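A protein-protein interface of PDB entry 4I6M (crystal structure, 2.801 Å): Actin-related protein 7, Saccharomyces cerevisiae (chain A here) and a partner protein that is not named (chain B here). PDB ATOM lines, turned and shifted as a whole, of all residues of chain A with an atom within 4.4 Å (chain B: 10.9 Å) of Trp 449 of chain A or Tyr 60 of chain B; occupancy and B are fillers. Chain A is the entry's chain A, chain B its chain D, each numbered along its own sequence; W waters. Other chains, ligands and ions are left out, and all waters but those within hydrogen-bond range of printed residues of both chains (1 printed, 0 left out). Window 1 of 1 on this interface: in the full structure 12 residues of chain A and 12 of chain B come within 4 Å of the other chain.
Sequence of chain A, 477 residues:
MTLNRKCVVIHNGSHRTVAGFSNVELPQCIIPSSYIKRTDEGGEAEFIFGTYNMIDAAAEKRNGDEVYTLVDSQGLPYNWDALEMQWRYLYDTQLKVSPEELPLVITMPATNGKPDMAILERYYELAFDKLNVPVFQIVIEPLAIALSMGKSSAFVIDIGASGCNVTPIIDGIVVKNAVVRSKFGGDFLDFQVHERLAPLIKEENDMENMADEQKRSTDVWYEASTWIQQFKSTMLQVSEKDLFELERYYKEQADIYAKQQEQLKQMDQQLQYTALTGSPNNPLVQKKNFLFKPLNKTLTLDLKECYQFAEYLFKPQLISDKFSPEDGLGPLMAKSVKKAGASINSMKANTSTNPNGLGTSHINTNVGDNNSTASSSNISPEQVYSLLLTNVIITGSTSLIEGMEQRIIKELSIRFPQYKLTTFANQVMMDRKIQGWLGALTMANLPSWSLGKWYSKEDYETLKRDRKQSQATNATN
O of Asn 4 of chain A sits at hydrogen-bond distance from OH of Tyr 60 of chain B (2.9 Å). The side-chain amide oxygen (OD1) of Asn 4 of chain A lies within hydrogen-bond range of the side-chain hydroxyl (OG1) of Thr 62 of chain B (2.8 Å). OE1 of Glu 101 of chain A lies within hydrogen-bond range of OH of Tyr 27 of chain B (3.1 Å). OE2 of Glu 101 of chain A is in salt-bridge range of NZ of Lys 61 of chain B.
The side-chain hydroxyl (OG) of Ser 448 of chain A lies within hydrogen-bond range of the side-chain hydroxyl (OG) of Ser 450 of chain A (2.8 Å). The backbone carbonyl oxygen of Leu 64 of chain B is in hydrogen-bond range of the backbone NH of Arg 26 of chain B, at 2.9 Å. O of Asp 28 of chain B sits at hydrogen-bond distance from N of Thr 62 of chain B. N of Tyr 56 of chain B sits at hydrogen-bond distance from O of Pro 32 of chain B, 2.8 Å away.
Among the printed residues, merely in contact across the chains: Asn 4 of chain A with Trp 63 of chain B (3.5 Å), Asn 4 of chain A with Leu 64 of chain B (3.9 Å), Arg 5 of chain A with Tyr 60 of chain B (3.4 Å), Glu 101 of chain A with Tyr 60 of chain B (3.3 Å), Pro 103 of chain A with Tyr 60 of chain B (3.6 Å), Trp 449 of chain A with Pro 32 of chain B (3.6 Å), Trp 449 of chain A with Tyr 56 of chain B (3.5 Å), Trp 449 of chain A with Phe 58 of chain B (3.5 Å), Trp 449 of chain A with Tyr 60 of chain B (3.4 Å) and Ser 450 of chain A with Tyr 56 of chain B (3.7 Å).
Tyr 60 of chain B touches just these residues of chain A: Asn 4 (2.9 Å), Arg 5 (3.4 Å), Glu 101 (3.3 Å), Pro 103 (3.6 Å) and Trp 449 (3.4 Å). Asn 4 of chain A touches just these residues of chain B: Tyr 60, Thr 62, Trp 63 and Leu 64. Arg 5 of chain A touches one residue of chain B. No residue of chain B comes within 4 Å of Leu 451 of chain A. No residue of chain B comes within 4 Å of Gly 452 of chain A. Of the printed residues of chain A, Thr 62 of chain B touches Asn 4 (2.8 Å). Printed residues of chain A within 4 Å of Tyr 56 of chain B: Trp 449 (3.5 Å) and Ser 450 (3.7 Å). Of the printed residues of chain A, Tyr 27 of chain B touches Glu 101. Of the printed residues of chain B, Pro 103 of chain A touches Tyr 60. Lys 55 of chain B touches none of the printed residues of chain A. The nearest printed residue of chain A that does not touch Tyr 27 of chain B is Pro 103 of chain A (7.9 Å).
Of the 11 printed residues of chain A, 6 touch a printed residue of chain B. Hydrophobic or aromatic side chains of chain A that line the printed part of chain B: Pro 103 and Trp 449. Printed residues of chain B that touch a printed residue of chain A: Tyr 27, Pro 32, Tyr 56, Phe 58, Tyr 60, Lys 61, Thr 62, Trp 63 and Leu 64. Hydrophobic or aromatic side chains of chain B within 4 Å of the printed part of chain A: Tyr 27, Pro 32, Tyr 56, Phe 58, Tyr 60 and Leu 64. Along chain B the printed residues that touch a printed residue of chain A span positions 27 to 64. Among the printed residues, Asp or Glu carboxylates within 4 Å of a Lys or Arg side-chain nitrogen of the other chain: Glu 101 of chain A with Lys 61 of chain B.
Water W1 bridges the side-chain amide oxygen of Asn 4 of chain A (2.7 Å) and the backbone carbonyl oxygen of Trp 63 of chain B (3.2 Å).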
ATOM      1  N   LEU A   3      18.534  18.660 -33.088  1.00  0.00           N
ATOM      2  CA  LEU A   3      17.682  18.623 -31.908  1.00  0.00           C
ATOM      3  C   LEU A   3      16.432  19.489 -32.067  1.00  0.00           C
ATOM      4  O   LEU A   3      16.440  20.529 -32.745  1.00  0.00           O
ATOM      5  CB  LEU A   3      18.463  19.072 -30.676  1.00  0.00           C
ATOM      6  CG  LEU A   3      19.642  18.221 -30.202  1.00  0.00           C
ATOM      7  CD1 LEU A   3      20.418  18.955 -29.116  1.00  0.00           C
ATOM      8  CD2 LEU A   3      19.151  16.901 -29.679  1.00  0.00           C
ATOM      9  N   ASN A   4      15.358  19.041 -31.430  1.00  0.00           N
ATOM     10  CA  ASN A   4      14.107  19.774 -31.411  1.00  0.00           C
ATOM     11  C   ASN A   4      14.131  20.814 -30.283  1.00  0.00           C
ATOM     12  O   ASN A   4      13.504  20.631 -29.228  1.00  0.00           O
ATOM     13  CB  ASN A   4      12.945  18.785 -31.255  1.00  0.00           C
ATOM     14  CG  ASN A   4      11.589  19.465 -31.140  1.00  0.00           C
ATOM     15  OD1 ASN A   4      11.417  20.633 -31.509  1.00  0.00           O
ATOM     16  ND2 ASN A   4      10.610  18.722 -30.631  1.00  0.00           N
ATOM     17  N   ARG A   5      14.883  21.893 -30.497  1.00  0.00           N
ATOM     18  CA  ARG A   5      14.959  22.971 -29.514  1.00  0.00           C
ATOM     19  C   ARG A   5      15.334  24.287 -30.166  1.00  0.00           C
ATOM     20  O   ARG A   5      15.815  24.336 -31.297  1.00  0.00           O
ATOM     21  CB  ARG A   5      15.964  22.660 -28.396  1.00  0.00           C
ATOM     22  CG  ARG A   5      17.382  22.837 -28.838  1.00  0.00           C
ATOM     23  CD  ARG A   5      18.400  22.623 -27.744  1.00  0.00           C
ATOM     24  NE  ARG A   5      19.729  22.531 -28.348  1.00  0.00           N
ATOM     25  CZ  ARG A   5      20.812  22.081 -27.728  1.00  0.00           C
ATOM     26  NH1 ARG A   5      20.739  21.685 -26.465  1.00  0.00           N
ATOM     27  NH2 ARG A   5      21.970  22.019 -28.370  1.00  0.00           N
ATOM     28  N   GLU A 101      10.715  29.496 -20.780  1.00  0.00           N
ATOM     29  CA  GLU A 101      10.414  28.505 -21.818  1.00  0.00           C
ATOM     30  C   GLU A 101      11.613  27.776 -22.442  1.00  0.00           C
ATOM     31  O   GLU A 101      11.565  26.558 -22.642  1.00  0.00           O
ATOM     32  CB  GLU A 101       9.550  29.114 -22.937  1.00  0.00           C
ATOM     33  CG  GLU A 101       8.438  30.020 -22.452  1.00  0.00           C
ATOM     34  CD  GLU A 101       7.283  30.123 -23.441  1.00  0.00           C
ATOM     35  OE1 GLU A 101       7.526  30.279 -24.663  1.00  0.00           O
ATOM     36  OE2 GLU A 101       6.122  30.033 -22.985  1.00  0.00           O
ATOM     37  N   PRO A 103      15.883  26.917 -23.532  1.00  0.00           N
ATOM     38  CA  PRO A 103      17.229  26.881 -22.976  1.00  0.00           C
ATOM     39  C   PRO A 103      18.036  28.147 -23.307  1.00  0.00           C
ATOM     40  O   PRO A 103      17.866  28.738 -24.375  1.00  0.00           O
ATOM     41  CB  PRO A 103      17.844  25.630 -23.622  1.00  0.00           C
ATOM     42  CG  PRO A 103      16.911  25.228 -24.709  1.00  0.00           C
ATOM     43  CD  PRO A 103      15.570  25.719 -24.321  1.00  0.00           C
ATOM     44  N   SER A 448      24.022  17.435 -30.271  1.00  0.00           N
ATOM     45  CA  SER A 448      23.827  16.535 -29.136  1.00  0.00           C
ATOM     46  C   SER A 448      23.838  17.299 -27.826  1.00  0.00           C
ATOM     47  O   SER A 448      24.616  18.232 -27.678  1.00  0.00           O
ATOM     48  CB  SER A 448      24.911  15.454 -29.133  1.00  0.00           C
ATOM     49  OG  SER A 448      24.736  14.542 -28.065  1.00  0.00           O
ATOM     50  N   TRP A 449      22.967  16.914 -26.887  1.00  0.00           N
ATOM     51  CA  TRP A 449      22.899  17.571 -25.571  1.00  0.00           C
ATOM     52  C   TRP A 449      24.150  17.307 -24.748  1.00  0.00           C
ATOM     53  O   TRP A 449      24.416  17.989 -23.758  1.00  0.00           O
ATOM     54  CB  TRP A 449      21.680  17.109 -24.766  1.00  0.00           C
ATOM     55  CG  TRP A 449      20.384  17.760 -25.143  1.00  0.00           C
ATOM     56  CD1 TRP A 449      19.431  17.274 -26.001  1.00  0.00           C
ATOM     57  CD2 TRP A 449      19.889  19.011 -24.664  1.00  0.00           C
ATOM     58  NE1 TRP A 449      18.375  18.148 -26.082  1.00  0.00           N
ATOM     59  CE2 TRP A 449      18.638  19.228 -25.276  1.00  0.00           C
ATOM     60  CE3 TRP A 449      20.384  19.976 -23.780  1.00  0.00           C
ATOM     61  CZ2 TRP A 449      17.882  20.372 -25.032  1.00  0.00           C
ATOM     62  CZ3 TRP A 449      19.637  21.104 -23.540  1.00  0.00           C
ATOM     63  CH2 TRP A 449      18.398  21.292 -24.161  1.00  0.00           C
ATOM     64  N   SER A 450      24.915  16.308 -25.167  1.00  0.00           N
ATOM     65  CA  SER A 450      26.084  15.861 -24.425  1.00  0.00           C
ATOM     66  C   SER A 450      27.327  16.654 -24.795  1.00  0.00           C
ATOM     67  O   SER A 450      28.391  16.446 -24.211  1.00  0.00           O
ATOM     68  CB  SER A 450      26.344  14.394 -24.731  1.00  0.00           C
ATOM     69  OG  SER A 450      26.732  14.254 -26.087  1.00  0.00           O
ATOM     70  N   LEU A 451      27.196  17.550 -25.769  1.00  0.00           N
ATOM     71  CA  LEU A 451      28.343  18.322 -26.234  1.00  0.00           C
ATOM     72  C   LEU A 451      28.701  19.501 -25.338  1.00  0.00           C
ATOM     73  O   LEU A 451      29.826  19.995 -25.378  1.00  0.00           O
ATOM     74  CB  LEU A 451      28.161  18.761 -27.677  1.00  0.00           C
ATOM     75  CG  LEU A 451      28.190  17.545 -28.611  1.00  0.00           C
ATOM     76  CD1 LEU A 451      28.162  17.961 -30.067  1.00  0.00           C
ATOM     77  CD2 LEU A 451      29.417  16.731 -28.340  1.00  0.00           C
ATOM     78  N   GLY A 452      27.764  19.931 -24.503  1.00  0.00           N
ATOM     79  CA  GLY A 452      28.057  20.997 -23.562  1.00  0.00           C
ATOM     80  C   GLY A 452      27.571  20.721 -22.156  1.00  0.00           C
ATOM     81  O   GLY A 452      26.629  19.960 -21.952  1.00  0.00           O
ATOM     82  N   TRP A 454      25.380  21.505 -19.319  1.00  0.00           N
ATOM     83  CA  TRP A 454      24.134  22.230 -19.194  1.00  0.00           C
ATOM     84  C   TRP A 454      23.710  22.253 -17.742  1.00  0.00           C
ATOM     85  O   TRP A 454      23.338  21.234 -17.196  1.00  0.00           O
ATOM     86  CB  TRP A 454      23.064  21.564 -20.041  1.00  0.00           C
ATOM     87  CG  TRP A 454      23.218  21.788 -21.531  1.00  0.00           C
ATOM     88  CD1 TRP A 454      23.891  21.002 -22.416  1.00  0.00           C
ATOM     89  CD2 TRP A 454      22.653  22.859 -22.301  1.00  0.00           C
ATOM     90  NE1 TRP A 454      23.782  21.516 -23.689  1.00  0.00           N
ATOM     91  CE2 TRP A 454      23.030  22.658 -23.642  1.00  0.00           C
ATOM     92  CE3 TRP A 454      21.874  23.974 -21.980  1.00  0.00           C
ATOM     93  CZ2 TRP A 454      22.657  23.522 -24.653  1.00  0.00           C
ATOM     94  CZ3 TRP A 454      21.504  24.833 -22.990  1.00  0.00           C
ATOM     95  CH2 TRP A 454      21.893  24.604 -24.310  1.00  0.00           C
ATOM     96  N   ARG B  26       1.725  20.672 -30.830  1.00  0.00           N
ATOM     97  CA  ARG B  26       1.392  21.460 -29.663  1.00  0.00           C
ATOM     98  C   ARG B  26       2.661  22.099 -29.142  1.00  0.00           C
ATOM     99  O   ARG B  26       3.759  21.649 -29.453  1.00  0.00           O
ATOM    100  CB  ARG B  26       0.720  20.592 -28.593  1.00  0.00           C
ATOM    101  CG  ARG B  26       1.626  19.639 -27.859  1.00  0.00           C
ATOM    102  CD  ARG B  26       0.830  18.813 -26.863  1.00  0.00           C
ATOM    103  NE  ARG B  26       1.707  18.084 -25.952  1.00  0.00           N
ATOM    104  CZ  ARG B  26       2.201  16.876 -26.200  1.00  0.00           C
ATOM    105  NH1 ARG B  26       1.901  16.253 -27.330  1.00  0.00           N
ATOM    106  NH2 ARG B  26       3.000  16.299 -25.319  1.00  0.00           N
ATOM    107  N   TYR B  27       2.518  23.164 -28.370  1.00  0.00           N
ATOM    108  CA  TYR B  27       3.686  23.833 -27.832  1.00  0.00           C
ATOM    109  C   TYR B  27       3.721  23.558 -26.348  1.00  0.00           C
ATOM    110  O   TYR B  27       2.971  24.150 -25.585  1.00  0.00           O
ATOM    111  CB  TYR B  27       3.633  25.333 -28.131  1.00  0.00           C
ATOM    112  CG  TYR B  27       4.891  26.065 -27.746  1.00  0.00           C
ATOM    113  CD1 TYR B  27       6.046  25.962 -28.516  1.00  0.00           C
ATOM    114  CD2 TYR B  27       4.931  26.850 -26.603  1.00  0.00           C
ATOM    115  CE1 TYR B  27       7.209  26.619 -28.144  1.00  0.00           C
ATOM    116  CE2 TYR B  27       6.084  27.504 -26.227  1.00  0.00           C
ATOM    117  CZ  TYR B  27       7.219  27.389 -26.999  1.00  0.00           C
ATOM    118  OH  TYR B  27       8.358  28.059 -26.618  1.00  0.00           O
ATOM    119  N   ASP B  28       4.585  22.639 -25.941  1.00  0.00           N
ATOM    120  CA  ASP B  28       4.508  22.083 -24.595  1.00  0.00           C
ATOM    121  C   ASP B  28       5.877  21.719 -24.041  1.00  0.00           C
ATOM    122  O   ASP B  28       6.881  21.751 -24.759  1.00  0.00           O
ATOM    123  CB  ASP B  28       3.618  20.836 -24.598  1.00  0.00           C
ATOM    124  CG  ASP B  28       2.934  20.593 -23.265  1.00  0.00           C
ATOM    125  OD1 ASP B  28       3.276  21.269 -22.271  1.00  0.00           O
ATOM    126  OD2 ASP B  28       2.052  19.714 -23.212  1.00  0.00           O
ATOM    127  N   TRP B  29       5.900  21.372 -22.756  1.00  0.00           N
ATOM    128  CA  TRP B  29       7.116  20.924 -22.080  1.00  0.00           C
ATOM    129  C   TRP B  29       7.656  19.616 -22.643  1.00  0.00           C
ATOM    130  O   TRP B  29       6.900  18.681 -22.924  1.00  0.00           O
ATOM    131  CB  TRP B  29       6.872  20.782 -20.573  1.00  0.00           C
ATOM    132  CG  TRP B  29       6.545  22.087 -19.914  1.00  0.00           C
ATOM    133  CD1 TRP B  29       5.332  22.492 -19.432  1.00  0.00           C
ATOM    134  CD2 TRP B  29       7.445  23.175 -19.693  1.00  0.00           C
ATOM    135  NE1 TRP B  29       5.426  23.758 -18.911  1.00  0.00           N
ATOM    136  CE2 TRP B  29       6.715  24.200 -19.064  1.00  0.00           C
ATOM    137  CE3 TRP B  29       8.799  23.380 -19.966  1.00  0.00           C
ATOM    138  CZ2 TRP B  29       7.294  25.406 -18.709  1.00  0.00           C
ATOM    139  CZ3 TRP B  29       9.366  24.574 -19.612  1.00  0.00           C
ATOM    140  CH2 TRP B  29       8.617  25.573 -18.990  1.00  0.00           C
ATOM    141  N   TYR B  30       8.973  19.572 -22.813  1.00  0.00           N
ATOM    142  CA  TYR B  30       9.664  18.394 -23.294  1.00  0.00           C
ATOM    143  C   TYR B  30      10.905  18.164 -22.452  1.00  0.00           C
ATOM    144  O   TYR B  30      11.561  19.111 -22.036  1.00  0.00           O
ATOM    145  CB  TYR B  30      10.057  18.559 -24.758  1.00  0.00           C
ATOM    146  CG  TYR B  30      10.826  17.366 -25.300  1.00  0.00           C
ATOM    147  CD1 TYR B  30      10.166  16.211 -25.679  1.00  0.00           C
ATOM    148  CD2 TYR B  30      12.208  17.394 -25.423  1.00  0.00           C
ATOM    149  CE1 TYR B  30      10.850  15.125 -26.167  1.00  0.00           C
ATOM    150  CE2 TYR B  30      12.900  16.310 -25.915  1.00  0.00           C
ATOM    151  CZ  TYR B  30      12.212  15.175 -26.285  1.00  0.00           C
ATOM    152  OH  TYR B  30      12.883  14.077 -26.772  1.00  0.00           O
ATOM    153  N   GLN B  31      11.233  16.902 -22.209  1.00  0.00           N
ATOM    154  CA  GLN B  31      12.346  16.550 -21.331  1.00  0.00           C
ATOM    155  C   GLN B  31      13.257  15.561 -22.033  1.00  0.00           C
ATOM    156  O   GLN B  31      12.974  14.361 -22.067  1.00  0.00           O
ATOM    157  CB  GLN B  31      11.812  15.939 -20.041  1.00  0.00           C
ATOM    158  CG  GLN B  31      12.871  15.551 -19.054  1.00  0.00           C
ATOM    159  CD  GLN B  31      12.297  14.814 -17.861  1.00  0.00           C
ATOM    160  OE1 GLN B  31      11.339  14.048 -17.987  1.00  0.00           O
ATOM    161  NE2 GLN B  31      12.878  15.043 -16.696  1.00  0.00           N
ATOM    162  N   PRO B  32      14.373  16.054 -22.578  1.00  0.00           N
ATOM    163  CA  PRO B  32      15.251  15.234 -23.413  1.00  0.00           C
ATOM    164  C   PRO B  32      15.894  14.102 -22.612  1.00  0.00           C
ATOM    165  O   PRO B  32      15.845  14.101 -21.378  1.00  0.00           O
ATOM    166  CB  PRO B  32      16.316  16.237 -23.863  1.00  0.00           C
ATOM    167  CG  PRO B  32      16.404  17.204 -22.744  1.00  0.00           C
ATOM    168  CD  PRO B  32      15.018  17.313 -22.170  1.00  0.00           C
ATOM    169  N   SER B  33      16.489  13.141 -23.306  1.00  0.00           N
ATOM    170  CA  SER B  33      17.187  12.055 -22.622  1.00  0.00           C
ATOM    171  C   SER B  33      18.537  11.763 -23.277  1.00  0.00           C
ATOM    172  O   SER B  33      18.818  12.263 -24.364  1.00  0.00           O
ATOM    173  CB  SER B  33      16.310  10.792 -22.533  1.00  0.00           C
ATOM    174  OG  SER B  33      15.719  10.470 -23.778  1.00  0.00           O
ATOM    175  N   LYS B  34      19.367  10.959 -22.611  1.00  0.00           N
ATOM    176  CA  LYS B  34      20.748  10.752 -23.045  1.00  0.00           C
ATOM    177  C   LYS B  34      20.917   9.711 -24.155  1.00  0.00           C
ATOM    178  O   LYS B  34      21.635   9.948 -25.136  1.00  0.00           O
ATOM    179  CB  LYS B  34      21.640  10.405 -21.852  1.00  0.00           C
ATOM    180  CG  LYS B  34      21.693  11.482 -20.775  1.00  0.00           C
ATOM    181  CD  LYS B  34      22.890  11.280 -19.857  1.00  0.00           C
ATOM    182  CE  LYS B  34      22.992  12.384 -18.813  1.00  0.00           C
ATOM    183  NZ  LYS B  34      22.235  12.059 -17.571  1.00  0.00           N
ATOM    184  N   GLU B  54      18.403   8.152 -17.608  1.00  0.00           N
ATOM    185  CA  GLU B  54      17.876   8.226 -18.972  1.00  0.00           C
ATOM    186  C   GLU B  54      17.507   9.666 -19.365  1.00  0.00           C
ATOM    187  O   GLU B  54      18.057  10.217 -20.316  1.00  0.00           O
ATOM    188  CB  GLU B  54      16.664   7.299 -19.138  1.00  0.00           C
ATOM    189  CG  GLU B  54      16.070   7.285 -20.545  1.00  0.00           C
ATOM    190  CD  GLU B  54      16.720   6.251 -21.452  1.00  0.00           C
ATOM    191  OE1 GLU B  54      17.225   5.237 -20.925  1.00  0.00           O
ATOM    192  OE2 GLU B  54      16.722   6.450 -22.689  1.00  0.00           O
ATOM    193  N   LYS B  55      16.584  10.271 -18.621  1.00  0.00           N
ATOM    194  CA  LYS B  55      16.106  11.620 -18.918  1.00  0.00           C
ATOM    195  C   LYS B  55      16.962  12.689 -18.243  1.00  0.00           C
ATOM    196  O   LYS B  55      17.285  12.565 -17.061  1.00  0.00           O
ATOM    197  CB  LYS B  55      14.646  11.778 -18.464  1.00  0.00           C
ATOM    198  CG  LYS B  55      13.626  10.869 -19.172  1.00  0.00           C
ATOM    199  CD  LYS B  55      13.491  11.206 -20.654  1.00  0.00           C
ATOM    200  CE  LYS B  55      12.048  11.514 -21.048  1.00  0.00           C
ATOM    201  NZ  LYS B  55      11.939  11.970 -22.468  1.00  0.00           N
ATOM    202  N   TYR B  56      17.320  13.739 -18.984  1.00  0.00           N
ATOM    203  CA  TYR B  56      17.993  14.893 -18.381  1.00  0.00           C
ATOM    204  C   TYR B  56      17.050  15.514 -17.352  1.00  0.00           C
ATOM    205  O   TYR B  56      15.834  15.385 -17.477  1.00  0.00           O
ATOM    206  CB  TYR B  56      18.395  15.931 -19.439  1.00  0.00           C
ATOM    207  CG  TYR B  56      19.591  15.549 -20.305  1.00  0.00           C
ATOM    208  CD1 TYR B  56      20.890  15.862 -19.913  1.00  0.00           C
ATOM    209  CD2 TYR B  56      19.417  14.892 -21.521  1.00  0.00           C
ATOM    210  CE1 TYR B  56      21.983  15.513 -20.700  1.00  0.00           C
ATOM    211  CE2 TYR B  56      20.506  14.544 -22.314  1.00  0.00           C
ATOM    212  CZ  TYR B  56      21.787  14.856 -21.898  1.00  0.00           C
ATOM    213  OH  TYR B  56      22.867  14.508 -22.684  1.00  0.00           O
ATOM    214  N   PRO B  57      17.603  16.169 -16.320  1.00  0.00           N
ATOM    215  CA  PRO B  57      16.821  16.760 -15.220  1.00  0.00           C
ATOM    216  C   PRO B  57      15.950  17.956 -15.609  1.00  0.00           C
ATOM    217  O   PRO B  57      15.118  18.372 -14.806  1.00  0.00           O
ATOM    218  CB  PRO B  57      17.898  17.239 -14.235  1.00  0.00           C
ATOM    219  CG  PRO B  57      19.125  16.486 -14.594  1.00  0.00           C
ATOM    220  CD  PRO B  57      19.051  16.256 -16.073  1.00  0.00           C
ATOM    221  N   PHE B  58      16.129  18.503 -16.804  1.00  0.00           N
ATOM    222  CA  PHE B  58      15.477  19.762 -17.143  1.00  0.00           C
ATOM    223  C   PHE B  58      14.343  19.642 -18.153  1.00  0.00           C
ATOM    224  O   PHE B  58      14.180  18.621 -18.810  1.00  0.00           O
ATOM    225  CB  PHE B  58      16.516  20.755 -17.650  1.00  0.00           C
ATOM    226  CG  PHE B  58      17.483  20.157 -18.615  1.00  0.00           C
ATOM    227  CD1 PHE B  58      17.187  20.103 -19.964  1.00  0.00           C
ATOM    228  CD2 PHE B  58      18.683  19.631 -18.170  1.00  0.00           C
ATOM    229  CE1 PHE B  58      18.072  19.547 -20.859  1.00  0.00           C
ATOM    230  CE2 PHE B  58      19.576  19.071 -19.058  1.00  0.00           C
ATOM    231  CZ  PHE B  58      19.268  19.031 -20.408  1.00  0.00           C
ATOM    232  N   ARG B  59      13.565  20.714 -18.258  1.00  0.00           N
ATOM    233  CA  ARG B  59      12.469  20.819 -19.205  1.00  0.00           C
ATOM    234  C   ARG B  59      12.712  22.005 -20.126  1.00  0.00           C
ATOM    235  O   ARG B  59      13.586  22.827 -19.881  1.00  0.00           O
ATOM    236  CB  ARG B  59      11.175  21.112 -18.468  1.00  0.00           C
ATOM    237  CG  ARG B  59      10.400  19.925 -17.987  1.00  0.00           C
ATOM    238  CD  ARG B  59       9.106  20.410 -17.347  1.00  0.00           C
ATOM    239  NE  ARG B  59       9.282  21.748 -16.788  1.00  0.00           N
ATOM    240  CZ  ARG B  59       8.361  22.393 -16.084  1.00  0.00           C
ATOM    241  NH1 ARG B  59       7.189  21.820 -15.848  1.00  0.00           N
ATOM    242  NH2 ARG B  59       8.614  23.609 -15.617  1.00  0.00           N
ATOM    243  N   TYR B  60      11.912  22.104 -21.176  1.00  0.00           N
ATOM    244  CA  TYR B  60      11.854  23.310 -21.968  1.00  0.00           C
ATOM    245  C   TYR B  60      10.702  23.203 -22.950  1.00  0.00           C
ATOM    246  O   TYR B  60      10.302  22.106 -23.318  1.00  0.00           O
ATOM    247  CB  TYR B  60      13.181  23.579 -22.671  1.00  0.00           C
ATOM    248  CG  TYR B  60      13.555  22.590 -23.728  1.00  0.00           C
ATOM    249  CD1 TYR B  60      14.215  21.410 -23.402  1.00  0.00           C
ATOM    250  CD2 TYR B  60      13.269  22.843 -25.065  1.00  0.00           C
ATOM    251  CE1 TYR B  60      14.573  20.505 -24.384  1.00  0.00           C
ATOM    252  CE2 TYR B  60      13.618  21.942 -26.059  1.00  0.00           C
ATOM    253  CZ  TYR B  60      14.266  20.780 -25.711  1.00  0.00           C
ATOM    254  OH  TYR B  60      14.598  19.892 -26.693  1.00  0.00           O
ATOM    255  N   LYS B  61      10.136  24.336 -23.347  1.00  0.00           N
ATOM    256  CA  LYS B  61       9.012  24.288 -24.257  1.00  0.00           C
ATOM    257  C   LYS B  61       9.527  24.071 -25.667  1.00  0.00           C
ATOM    258  O   LYS B  61      10.582  24.569 -26.047  1.00  0.00           O
ATOM    259  CB  LYS B  61       8.192  25.574 -24.188  1.00  0.00           C
ATOM    260  CG  LYS B  61       7.632  25.893 -22.817  1.00  0.00           C
ATOM    261  CD  LYS B  61       6.564  24.913 -22.397  1.00  0.00           C
ATOM    262  CE  LYS B  61       5.332  25.633 -21.892  1.00  0.00           C
ATOM    263  NZ  LYS B  61       4.773  26.517 -22.956  1.00  0.00           N
ATOM    264  N   THR B  62       8.786  23.306 -26.448  1.00  0.00           N
ATOM    265  CA  THR B  62       9.093  23.197 -27.856  1.00  0.00           C
ATOM    266  C   THR B  62       7.825  22.751 -28.581  1.00  0.00           C
ATOM    267  O   THR B  62       6.807  22.462 -27.950  1.00  0.00           O
ATOM    268  CB  THR B  62      10.247  22.224 -28.098  1.00  0.00           C
ATOM    269  OG1 THR B  62      10.755  22.404 -29.421  1.00  0.00           O
ATOM    270  CG2 THR B  62       9.780  20.781 -27.931  1.00  0.00           C
ATOM    271  N   TRP B  63       7.879  22.737 -29.904  1.00  0.00           N
ATOM    272  CA  TRP B  63       6.792  22.200 -30.701  1.00  0.00           C
ATOM    273  C   TRP B  63       6.887  20.689 -30.901  1.00  0.00           C
ATOM    274  O   TRP B  63       7.615  20.213 -31.775  1.00  0.00           O
ATOM    275  CB  TRP B  63       6.762  22.885 -32.056  1.00  0.00           C
ATOM    276  CG  TRP B  63       6.261  24.264 -31.979  1.00  0.00           C
ATOM    277  CD1 TRP B  63       7.002  25.407 -31.921  1.00  0.00           C
ATOM    278  CD2 TRP B  63       4.897  24.666 -31.946  1.00  0.00           C
ATOM    279  NE1 TRP B  63       6.181  26.492 -31.868  1.00  0.00           N
ATOM    280  CE2 TRP B  63       4.878  26.061 -31.877  1.00  0.00           C
ATOM    281  CE3 TRP B  63       3.686  23.977 -31.973  1.00  0.00           C
ATOM    282  CZ2 TRP B  63       3.696  26.780 -31.834  1.00  0.00           C
ATOM    283  CZ3 TRP B  63       2.524  24.688 -31.926  1.00  0.00           C
ATOM    284  CH2 TRP B  63       2.531  26.071 -31.858  1.00  0.00           C
ATOM    285  N   LEU B  64       6.125  19.952 -30.099  1.00  0.00           N
ATOM    286  CA  LEU B  64       6.016  18.505 -30.211  1.00  0.00           C
ATOM    287  C   LEU B  64       4.847  18.053 -31.109  1.00  0.00           C
ATOM    288  O   LEU B  64       3.746  18.599 -31.043  1.00  0.00           O
ATOM    289  CB  LEU B  64       5.808  17.914 -28.824  1.00  0.00           C
ATOM    290  CG  LEU B  64       6.813  18.261 -27.738  1.00  0.00           C
ATOM    291  CD1 LEU B  64       6.229  17.959 -26.372  1.00  0.00           C
ATOM    292  CD2 LEU B  64       8.075  17.483 -27.953  1.00  0.00           C
HETATM  293  O   HOH W   1       9.980  21.396 -33.607  1.00  0.00           O
